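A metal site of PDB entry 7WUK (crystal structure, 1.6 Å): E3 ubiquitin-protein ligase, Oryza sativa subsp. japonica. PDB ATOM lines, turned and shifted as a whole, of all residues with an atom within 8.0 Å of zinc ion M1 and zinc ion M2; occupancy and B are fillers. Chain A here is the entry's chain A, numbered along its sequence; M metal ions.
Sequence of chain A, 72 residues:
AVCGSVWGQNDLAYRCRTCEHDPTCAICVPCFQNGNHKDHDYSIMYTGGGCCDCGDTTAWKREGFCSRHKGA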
ATOM      1  N   VAL A   2      -6.799 -28.832  24.967  1.00  0.00           N
ATOM      2  CA  VAL A   2      -8.246 -29.269  24.730  1.00  0.00           C
ATOM      3  C   VAL A   2      -9.057 -28.818  25.957  1.00  0.00           C
ATOM      4  O   VAL A   2      -8.652 -29.112  27.103  1.00  0.00           O
ATOM      5  CB  VAL A   2      -8.427 -30.791  24.554  1.00  0.00           C
ATOM      6  CG1 VAL A   2      -9.904 -31.219  24.612  1.00  0.00           C
ATOM      7  CG2 VAL A   2      -7.814 -31.303  23.252  1.00  0.00           C
ATOM      8  N   CYS A   3     -10.215 -28.189  25.732  1.00  0.00           N
ATOM      9  CA  CYS A   3     -11.065 -27.676  26.817  1.00  0.00           C
ATOM     10  C   CYS A   3     -11.426 -28.806  27.779  1.00  0.00           C
ATOM     11  O   CYS A   3     -11.874 -29.868  27.353  1.00  0.00           O
ATOM     12  CB  CYS A   3     -12.343 -27.064  26.251  1.00  0.00           C
ATOM     13  SG  CYS A   3     -13.387 -26.346  27.549  1.00  0.00           S
ATOM     14  N   GLY A   4     -11.257 -28.541  29.074  1.00  0.00           N
ATOM     15  CA  GLY A   4     -11.547 -29.485  30.157  1.00  0.00           C
ATOM     16  C   GLY A   4     -12.963 -29.375  30.703  1.00  0.00           C
ATOM     17  O   GLY A   4     -13.282 -30.054  31.699  1.00  0.00           O
ATOM     18  N   SER A   5     -13.829 -28.588  30.083  1.00  0.00           N
ATOM     19  CA  SER A   5     -15.191 -28.327  30.604  1.00  0.00           C
ATOM     20  C   SER A   5     -16.047 -29.587  30.558  1.00  0.00           C
ATOM     21  O   SER A   5     -16.010 -30.272  29.555  1.00  0.00           O
ATOM     22  CB  SER A   5     -15.864 -27.192  29.861  1.00  0.00           C
ATOM     23  OG  SER A   5     -17.212 -27.100  30.275  1.00  0.00           O
ATOM     24  N   VAL A   6     -16.762 -29.870  31.635  1.00  0.00           N
ATOM     25  CA  VAL A   6     -17.778 -30.957  31.674  1.00  0.00           C
ATOM     26  C   VAL A   6     -19.094 -30.288  32.073  1.00  0.00           C
ATOM     27  O   VAL A   6     -19.099 -29.338  32.880  1.00  0.00           O
ATOM     28  CB  VAL A   6     -17.385 -32.112  32.609  1.00  0.00           C
ATOM     29  CG1 VAL A   6     -16.100 -32.792  32.111  1.00  0.00           C
ATOM     30  CG2 VAL A   6     -17.295 -31.644  34.039  1.00  0.00           C
ATOM     31  N   TRP A   7     -20.189 -30.824  31.597  1.00  0.00           N
ATOM     32  CA  TRP A   7     -21.520 -30.332  31.979  1.00  0.00           C
ATOM     33  C   TRP A   7     -22.518 -31.479  32.050  1.00  0.00           C
ATOM     34  O   TRP A   7     -22.228 -32.601  31.609  1.00  0.00           O
ATOM     35  CB  TRP A   7     -21.992 -29.224  31.034  1.00  0.00           C
ATOM     36  CG  TRP A   7     -22.242 -29.691  29.628  1.00  0.00           C
ATOM     37  CD1 TRP A   7     -23.420 -30.165  29.116  1.00  0.00           C
ATOM     38  CD2 TRP A   7     -21.327 -29.685  28.514  1.00  0.00           C
ATOM     39  NE1 TRP A   7     -23.282 -30.462  27.799  1.00  0.00           N
ATOM     40  CE2 TRP A   7     -22.008 -30.199  27.398  1.00  0.00           C
ATOM     41  CE3 TRP A   7     -19.988 -29.296  28.351  1.00  0.00           C
ATOM     42  CZ2 TRP A   7     -21.425 -30.332  26.154  1.00  0.00           C
ATOM     43  CZ3 TRP A   7     -19.438 -29.363  27.090  1.00  0.00           C
ATOM     44  CH2 TRP A   7     -20.125 -29.932  26.033  1.00  0.00           C
ATOM     45  N   ALA A  26     -19.941 -31.567  20.612  1.00  0.00           N
ATOM     46  CA  ALA A  26     -20.497 -30.373  21.256  1.00  0.00           C
ATOM     47  C   ALA A  26     -19.372 -29.589  21.886  1.00  0.00           C
ATOM     48  O   ALA A  26     -18.355 -30.193  22.263  1.00  0.00           O
ATOM     49  CB  ALA A  26     -21.536 -30.712  22.305  1.00  0.00           C
ATOM     50  N   ILE A  27     -19.610 -28.291  22.028  1.00  0.00           N
ATOM     51  CA  ILE A  27     -18.665 -27.406  22.758  1.00  0.00           C
ATOM     52  C   ILE A  27     -19.423 -26.614  23.805  1.00  0.00           C
ATOM     53  O   ILE A  27     -20.614 -26.352  23.649  1.00  0.00           O
ATOM     54  CB  ILE A  27     -17.818 -26.489  21.872  1.00  0.00           C
ATOM     55  CG1 ILE A  27     -18.638 -25.481  21.067  1.00  0.00           C
ATOM     56  CG2 ILE A  27     -16.921 -27.332  20.963  1.00  0.00           C
ATOM     57  CD1 ILE A  27     -17.773 -24.467  20.361  1.00  0.00           C
ATOM     58  N   CYS A  28     -18.732 -26.229  24.853  1.00  0.00           N
ATOM     59  CA  CYS A  28     -19.321 -25.474  25.980  1.00  0.00           C
ATOM     60  C   CYS A  28     -19.694 -24.051  25.534  1.00  0.00           C
ATOM     61  O   CYS A  28     -19.232 -23.549  24.515  1.00  0.00           O
ATOM     62  CB  CYS A  28     -18.391 -25.527  27.195  1.00  0.00           C
ATOM     63  SG  CYS A  28     -16.877 -24.544  27.026  1.00  0.00           S
ATOM     64  N   VAL A  29     -20.571 -23.438  26.308  1.00  0.00           N
ATOM     65  CA  VAL A  29     -21.049 -22.096  25.922  1.00  0.00           C
ATOM     66  C   VAL A  29     -19.839 -21.153  25.793  1.00  0.00           C
ATOM     67  O   VAL A  29     -19.733 -20.451  24.822  1.00  0.00           O
ATOM     68  CB  VAL A  29     -22.127 -21.604  26.896  1.00  0.00           C
ATOM     69  CG1 VAL A  29     -22.334 -20.101  26.721  1.00  0.00           C
ATOM     70  CG2 VAL A  29     -23.435 -22.351  26.682  1.00  0.00           C
ATOM     71  N   PRO A  30     -18.904 -21.072  26.768  1.00  0.00           N
ATOM     72  CA  PRO A  30     -17.784 -20.131  26.603  1.00  0.00           C
ATOM     73  C   PRO A  30     -16.912 -20.400  25.389  1.00  0.00           C
ATOM     74  O   PRO A  30     -16.473 -19.475  24.731  1.00  0.00           O
ATOM     75  CB  PRO A  30     -17.022 -20.212  27.920  1.00  0.00           C
ATOM     76  CG  PRO A  30     -17.939 -20.851  28.896  1.00  0.00           C
ATOM     77  CD  PRO A  30     -19.020 -21.568  28.137  1.00  0.00           C
ATOM     78  N   CYS A  31     -16.669 -21.675  25.068  1.00  0.00           N
ATOM     79  CA  CYS A  31     -15.876 -21.972  23.876  1.00  0.00           C
ATOM     80  C   CYS A  31     -16.636 -21.514  22.628  1.00  0.00           C
ATOM     81  O   CYS A  31     -15.996 -20.944  21.763  1.00  0.00           O
ATOM     82  CB  CYS A  31     -15.551 -23.442  23.813  1.00  0.00           C
ATOM     83  SG  CYS A  31     -14.200 -23.831  24.984  1.00  0.00           S
ATOM     84  N   PHE A  32     -17.942 -21.679  22.575  1.00  0.00           N
ATOM     85  CA  PHE A  32     -18.743 -21.147  21.451  1.00  0.00           C
ATOM     86  C   PHE A  32     -18.576 -19.631  21.378  1.00  0.00           C
ATOM     87  O   PHE A  32     -18.310 -19.096  20.263  1.00  0.00           O
ATOM     88  CB  PHE A  32     -20.215 -21.544  21.565  1.00  0.00           C
ATOM     89  CG  PHE A  32     -20.965 -21.034  20.369  1.00  0.00           C
ATOM     90  CD1 PHE A  32     -20.982 -21.766  19.185  1.00  0.00           C
ATOM     91  CD2 PHE A  32     -21.592 -19.814  20.419  1.00  0.00           C
ATOM     92  CE1 PHE A  32     -21.606 -21.244  18.062  1.00  0.00           C
ATOM     93  CE2 PHE A  32     -22.272 -19.313  19.309  1.00  0.00           C
ATOM     94  CZ  PHE A  32     -22.251 -20.033  18.143  1.00  0.00           C
ATOM     95  N   ASN A  34     -16.369 -17.643  22.393  1.00  0.00           N
ATOM     96  CA  ASN A  34     -14.992 -17.162  22.155  1.00  0.00           C
ATOM     97  C   ASN A  34     -14.471 -17.640  20.808  1.00  0.00           C
ATOM     98  O   ASN A  34     -13.281 -17.466  20.546  1.00  0.00           O
ATOM     99  CB  ASN A  34     -14.087 -17.544  23.332  1.00  0.00           C
ATOM    100  CG  ASN A  34     -14.340 -16.705  24.551  1.00  0.00           C
ATOM    101  OD1 ASN A  34     -14.265 -17.184  25.691  1.00  0.00           O
ATOM    102  ND2 ASN A  34     -14.494 -15.410  24.312  1.00  0.00           N
ATOM    103  N   GLY A  35     -15.307 -18.268  19.976  1.00  0.00           N
ATOM    104  CA  GLY A  35     -14.952 -18.707  18.619  1.00  0.00           C
ATOM    105  C   GLY A  35     -15.787 -18.017  17.562  1.00  0.00           C
ATOM    106  O   GLY A  35     -16.622 -17.136  17.868  1.00  0.00           O
ATOM    107  N   CYS A  51     -18.585 -33.628  27.629  1.00  0.00           N
ATOM    108  CA  CYS A  51     -17.248 -33.009  27.755  1.00  0.00           C
ATOM    109  C   CYS A  51     -17.049 -32.142  26.512  1.00  0.00           C
ATOM    110  O   CYS A  51     -17.501 -32.480  25.451  1.00  0.00           O
ATOM    111  CB  CYS A  51     -16.091 -33.995  27.768  1.00  0.00           C
ATOM    112  SG  CYS A  51     -16.123 -35.088  29.203  1.00  0.00           S
ATOM    113  N   CYS A  52     -16.356 -31.037  26.656  1.00  0.00           N
ATOM    114  CA  CYS A  52     -16.195 -30.108  25.519  1.00  0.00           C
ATOM    115  C   CYS A  52     -15.237 -30.684  24.473  1.00  0.00           C
ATOM    116  O   CYS A  52     -14.190 -31.263  24.880  1.00  0.00           O
ATOM    117  CB  CYS A  52     -15.649 -28.794  26.046  1.00  0.00           C
ATOM    118  SG  CYS A  52     -15.646 -27.489  24.795  1.00  0.00           S
ATOM    119  N   ASP A  53     -15.521 -30.458  23.192  1.00  0.00           N
ATOM    120  CA  ASP A  53     -14.699 -30.932  22.053  1.00  0.00           C
ATOM    121  C   ASP A  53     -13.762 -29.824  21.559  1.00  0.00           C
ATOM    122  O   ASP A  53     -13.010 -30.090  20.574  1.00  0.00           O
ATOM    123  CB  ASP A  53     -15.593 -31.441  20.929  1.00  0.00           C
ATOM    124  CG  ASP A  53     -16.211 -32.778  21.309  1.00  0.00           C
ATOM    125  OD1 ASP A  53     -15.515 -33.561  21.993  1.00  0.00           O
ATOM    126  OD2 ASP A  53     -17.371 -33.020  20.978  1.00  0.00           O
ATOM    127  N   CYS A  54     -13.811 -28.626  22.148  1.00  0.00           N
ATOM    128  CA  CYS A  54     -12.995 -27.487  21.639  1.00  0.00           C
ATOM    129  C   CYS A  54     -11.504 -27.770  21.826  1.00  0.00           C
ATOM    130  O   CYS A  54     -11.072 -28.035  22.961  1.00  0.00           O
ATOM    131  CB  CYS A  54     -13.354 -26.227  22.387  1.00  0.00           C
ATOM    132  SG  CYS A  54     -12.530 -24.775  21.714  1.00  0.00           S
ATOM    133  N   GLY A  55     -10.752 -27.672  20.750  1.00  0.00           N
ATOM    134  CA  GLY A  55      -9.305 -28.011  20.773  1.00  0.00           C
ATOM    135  C   GLY A  55      -9.003 -29.411  20.333  1.00  0.00           C
ATOM    136  O   GLY A  55      -7.799 -29.676  20.052  1.00  0.00           O
ATOM    137  N   ASP A  56     -10.012 -30.303  20.255  1.00  0.00           N
ATOM    138  CA  ASP A  56      -9.842 -31.729  19.892  1.00  0.00           C
ATOM    139  C   ASP A  56      -9.955 -31.883  18.375  1.00  0.00           C
ATOM    140  O   ASP A  56     -11.094 -31.917  17.855  1.00  0.00           O
ATOM    141  CB  ASP A  56     -10.865 -32.606  20.604  1.00  0.00           C
ATOM    142  CG  ASP A  56     -10.649 -34.092  20.349  1.00  0.00           C
ATOM    143  OD1 ASP A  56      -9.759 -34.446  19.528  1.00  0.00           O
ATOM    144  OD2 ASP A  56     -11.414 -34.888  20.970  1.00  0.00           O
ATOM    145  N   TRP A  60     -13.529 -31.945  16.151  1.00  0.00           N
ATOM    146  CA  TRP A  60     -13.995 -30.573  15.827  1.00  0.00           C
ATOM    147  C   TRP A  60     -13.009 -29.933  14.837  1.00  0.00           C
ATOM    148  O   TRP A  60     -11.779 -30.015  15.045  1.00  0.00           O
ATOM    149  CB  TRP A  60     -14.054 -29.734  17.103  1.00  0.00           C
ATOM    150  CG  TRP A  60     -14.956 -28.548  17.104  1.00  0.00           C
ATOM    151  CD1 TRP A  60     -14.581 -27.248  16.949  1.00  0.00           C
ATOM    152  CD2 TRP A  60     -16.380 -28.538  17.342  1.00  0.00           C
ATOM    153  NE1 TRP A  60     -15.654 -26.422  17.122  1.00  0.00           N
ATOM    154  CE2 TRP A  60     -16.776 -27.182  17.337  1.00  0.00           C
ATOM    155  CE3 TRP A  60     -17.345 -29.520  17.544  1.00  0.00           C
ATOM    156  CZ2 TRP A  60     -18.083 -26.796  17.549  1.00  0.00           C
ATOM    157  CZ3 TRP A  60     -18.654 -29.130  17.715  1.00  0.00           C
ATOM    158  CH2 TRP A  60     -19.014 -27.782  17.714  1.00  0.00           C
ATOM    159  N   GLY A  64     -13.043 -23.891  14.044  1.00  0.00           N
ATOM    160  CA  GLY A  64     -14.096 -23.772  15.055  1.00  0.00           C
ATOM    161  C   GLY A  64     -13.566 -23.780  16.478  1.00  0.00           C
ATOM    162  O   GLY A  64     -14.392 -23.745  17.356  1.00  0.00           O
ATOM    163  N   PHE A  65     -12.251 -23.778  16.693  1.00  0.00           N
ATOM    164  CA  PHE A  65     -11.676 -23.696  18.049  1.00  0.00           C
ATOM    165  C   PHE A  65     -11.810 -22.270  18.563  1.00  0.00           C
ATOM    166  O   PHE A  65     -11.612 -21.271  17.759  1.00  0.00           O
ATOM    167  CB  PHE A  65     -10.193 -24.099  18.072  1.00  0.00           C
ATOM    168  CG  PHE A  65      -9.880 -25.531  17.748  1.00  0.00           C
ATOM    169  CD1 PHE A  65     -10.871 -26.487  17.585  1.00  0.00           C
ATOM    170  CD2 PHE A  65      -8.564 -25.936  17.583  1.00  0.00           C
ATOM    171  CE1 PHE A  65     -10.553 -27.800  17.283  1.00  0.00           C
ATOM    172  CE2 PHE A  65      -8.254 -27.258  17.302  1.00  0.00           C
ATOM    173  CZ  PHE A  65      -9.252 -28.194  17.164  1.00  0.00           C
ATOM    174  N   CYS A  66     -12.061 -22.118  19.852  1.00  0.00           N
ATOM    175  CA  CYS A  66     -12.056 -20.751  20.445  1.00  0.00           C
ATOM    176  C   CYS A  66     -10.637 -20.203  20.565  1.00  0.00           C
ATOM    177  O   CYS A  66      -9.654 -20.910  20.354  1.00  0.00           O
ATOM    178  CB  CYS A  66     -12.805 -20.700  21.769  1.00  0.00           C
ATOM    179  SG  CYS A  66     -11.814 -21.317  23.166  1.00  0.00           S
ATOM    180  N   SER A  67     -10.575 -18.919  20.884  1.00  0.00           N
ATOM    181  CA  SER A  67      -9.318 -18.157  21.022  1.00  0.00           C
ATOM    182  C   SER A  67      -8.413 -18.846  22.049  1.00  0.00           C
ATOM    183  O   SER A  67      -7.188 -18.757  21.931  1.00  0.00           O
ATOM    184  CB  SER A  67      -9.639 -16.734  21.368  1.00  0.00           C
ATOM    185  OG  SER A  67     -10.511 -16.656  22.490  1.00  0.00           O
ATOM    186  N   ARG A  68      -8.979 -19.521  23.044  1.00  0.00           N
ATOM    187  CA  ARG A  68      -8.263 -20.017  24.248  1.00  0.00           C
ATOM    188  C   ARG A  68      -7.736 -21.440  24.019  1.00  0.00           C
ATOM    189  O   ARG A  68      -6.827 -21.827  24.768  1.00  0.00           O
ATOM    190  CB  ARG A  68      -9.208 -19.831  25.443  1.00  0.00           C
ATOM    191  CG  ARG A  68      -9.798 -18.423  25.532  1.00  0.00           C
ATOM    192  CD  ARG A  68     -10.714 -18.160  26.733  1.00  0.00           C
ATOM    193  NE  ARG A  68      -9.990 -18.368  27.974  1.00  0.00           N
ATOM    194  CZ  ARG A  68      -9.974 -19.495  28.670  1.00  0.00           C
ATOM    195  NH1 ARG A  68     -10.697 -20.535  28.287  1.00  0.00           N
ATOM    196  NH2 ARG A  68      -9.209 -19.596  29.733  1.00  0.00           N
ATOM    197  N   HIS A  69      -8.217 -22.209  23.016  1.00  0.00           N
ATOM    198  CA  HIS A  69      -7.784 -23.613  22.758  1.00  0.00           C
ATOM    199  C   HIS A  69      -7.475 -23.847  21.266  1.00  0.00           C
ATOM    200  O   HIS A  69      -6.893 -22.952  20.673  1.00  0.00           O
ATOM    201  CB  HIS A  69      -8.844 -24.643  23.200  1.00  0.00           C
ATOM    202  CG  HIS A  69      -9.449 -24.397  24.538  1.00  0.00           C
ATOM    203  ND1 HIS A  69      -8.781 -24.603  25.765  1.00  0.00           N
ATOM    204  CD2 HIS A  69     -10.690 -24.008  24.871  1.00  0.00           C
ATOM    205  CE1 HIS A  69      -9.573 -24.252  26.758  1.00  0.00           C
ATOM    206  NE2 HIS A  69     -10.755 -23.922  26.234  1.00  0.00           N
HETATM  207 ZN    ZN M   1     -15.061 -25.703  26.148  1.00  0.00          ZN
HETATM  208 ZN    ZN M   2     -12.260 -23.518  23.578  1.00  0.00          ZN
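Residues that only touch zinc ion M2: His 69. Within 4 Å of zinc ion M2: Cys 31, Cys 54, Cys 66 and His 69. Along chain A the residues within 4 Å of zinc ion M2 span positions 31 to 69.
Zinc ion M2 is bound by the side-chain sulfur (SG) of Cys 54 (2.3 Å), the side-chain sulfur (SG) of Cys 66 (2.3 Å) and the side-chain sulfur (SG) of Cys 31 (2.4 Å). Zinc ion M2 has three donor atoms within binding distance.
The backbone carbonyl oxygen (O) of Cys 54 lies within hydrogen-bond range of the backbone NH (N) of Cys 3. NE2 of His 69 sits close to SG of Cys 31, at 3.7 Å. The side-chain sulfur (SG) of Cys 3 lies close to the backbone NH (N) of Ser 5, 3.4 Å away. N of His 69 sits close to SG of Cys 66, 3.7 Å away. N of Arg 68 sits close to SG of Cys 66, at 3.4 Å. The side-chain sulfur of Cys 52 lies close to the backbone NH of Cys 54 (3.4 Å). N of Cys 52 lies within hydrogen-bond range of O of Ser 5, at 3.0 Å.
SG of Cys 3 binds zinc ion M1, 2.3 Å away. Zinc ion M1 is bound by SG of Cys 52 (2.3 Å). SG of Cys 28 binds zinc ion M1, at 2.3 Å. The side-chain sulfur (SG) of Cys 31 is bound to zinc ion M1 (2.4 Å). Zinc ion M1 has four donor atoms within binding distance.
The nearest printed residue that does not touch zinc ion M1 is Ser 5 (4.1 Å).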
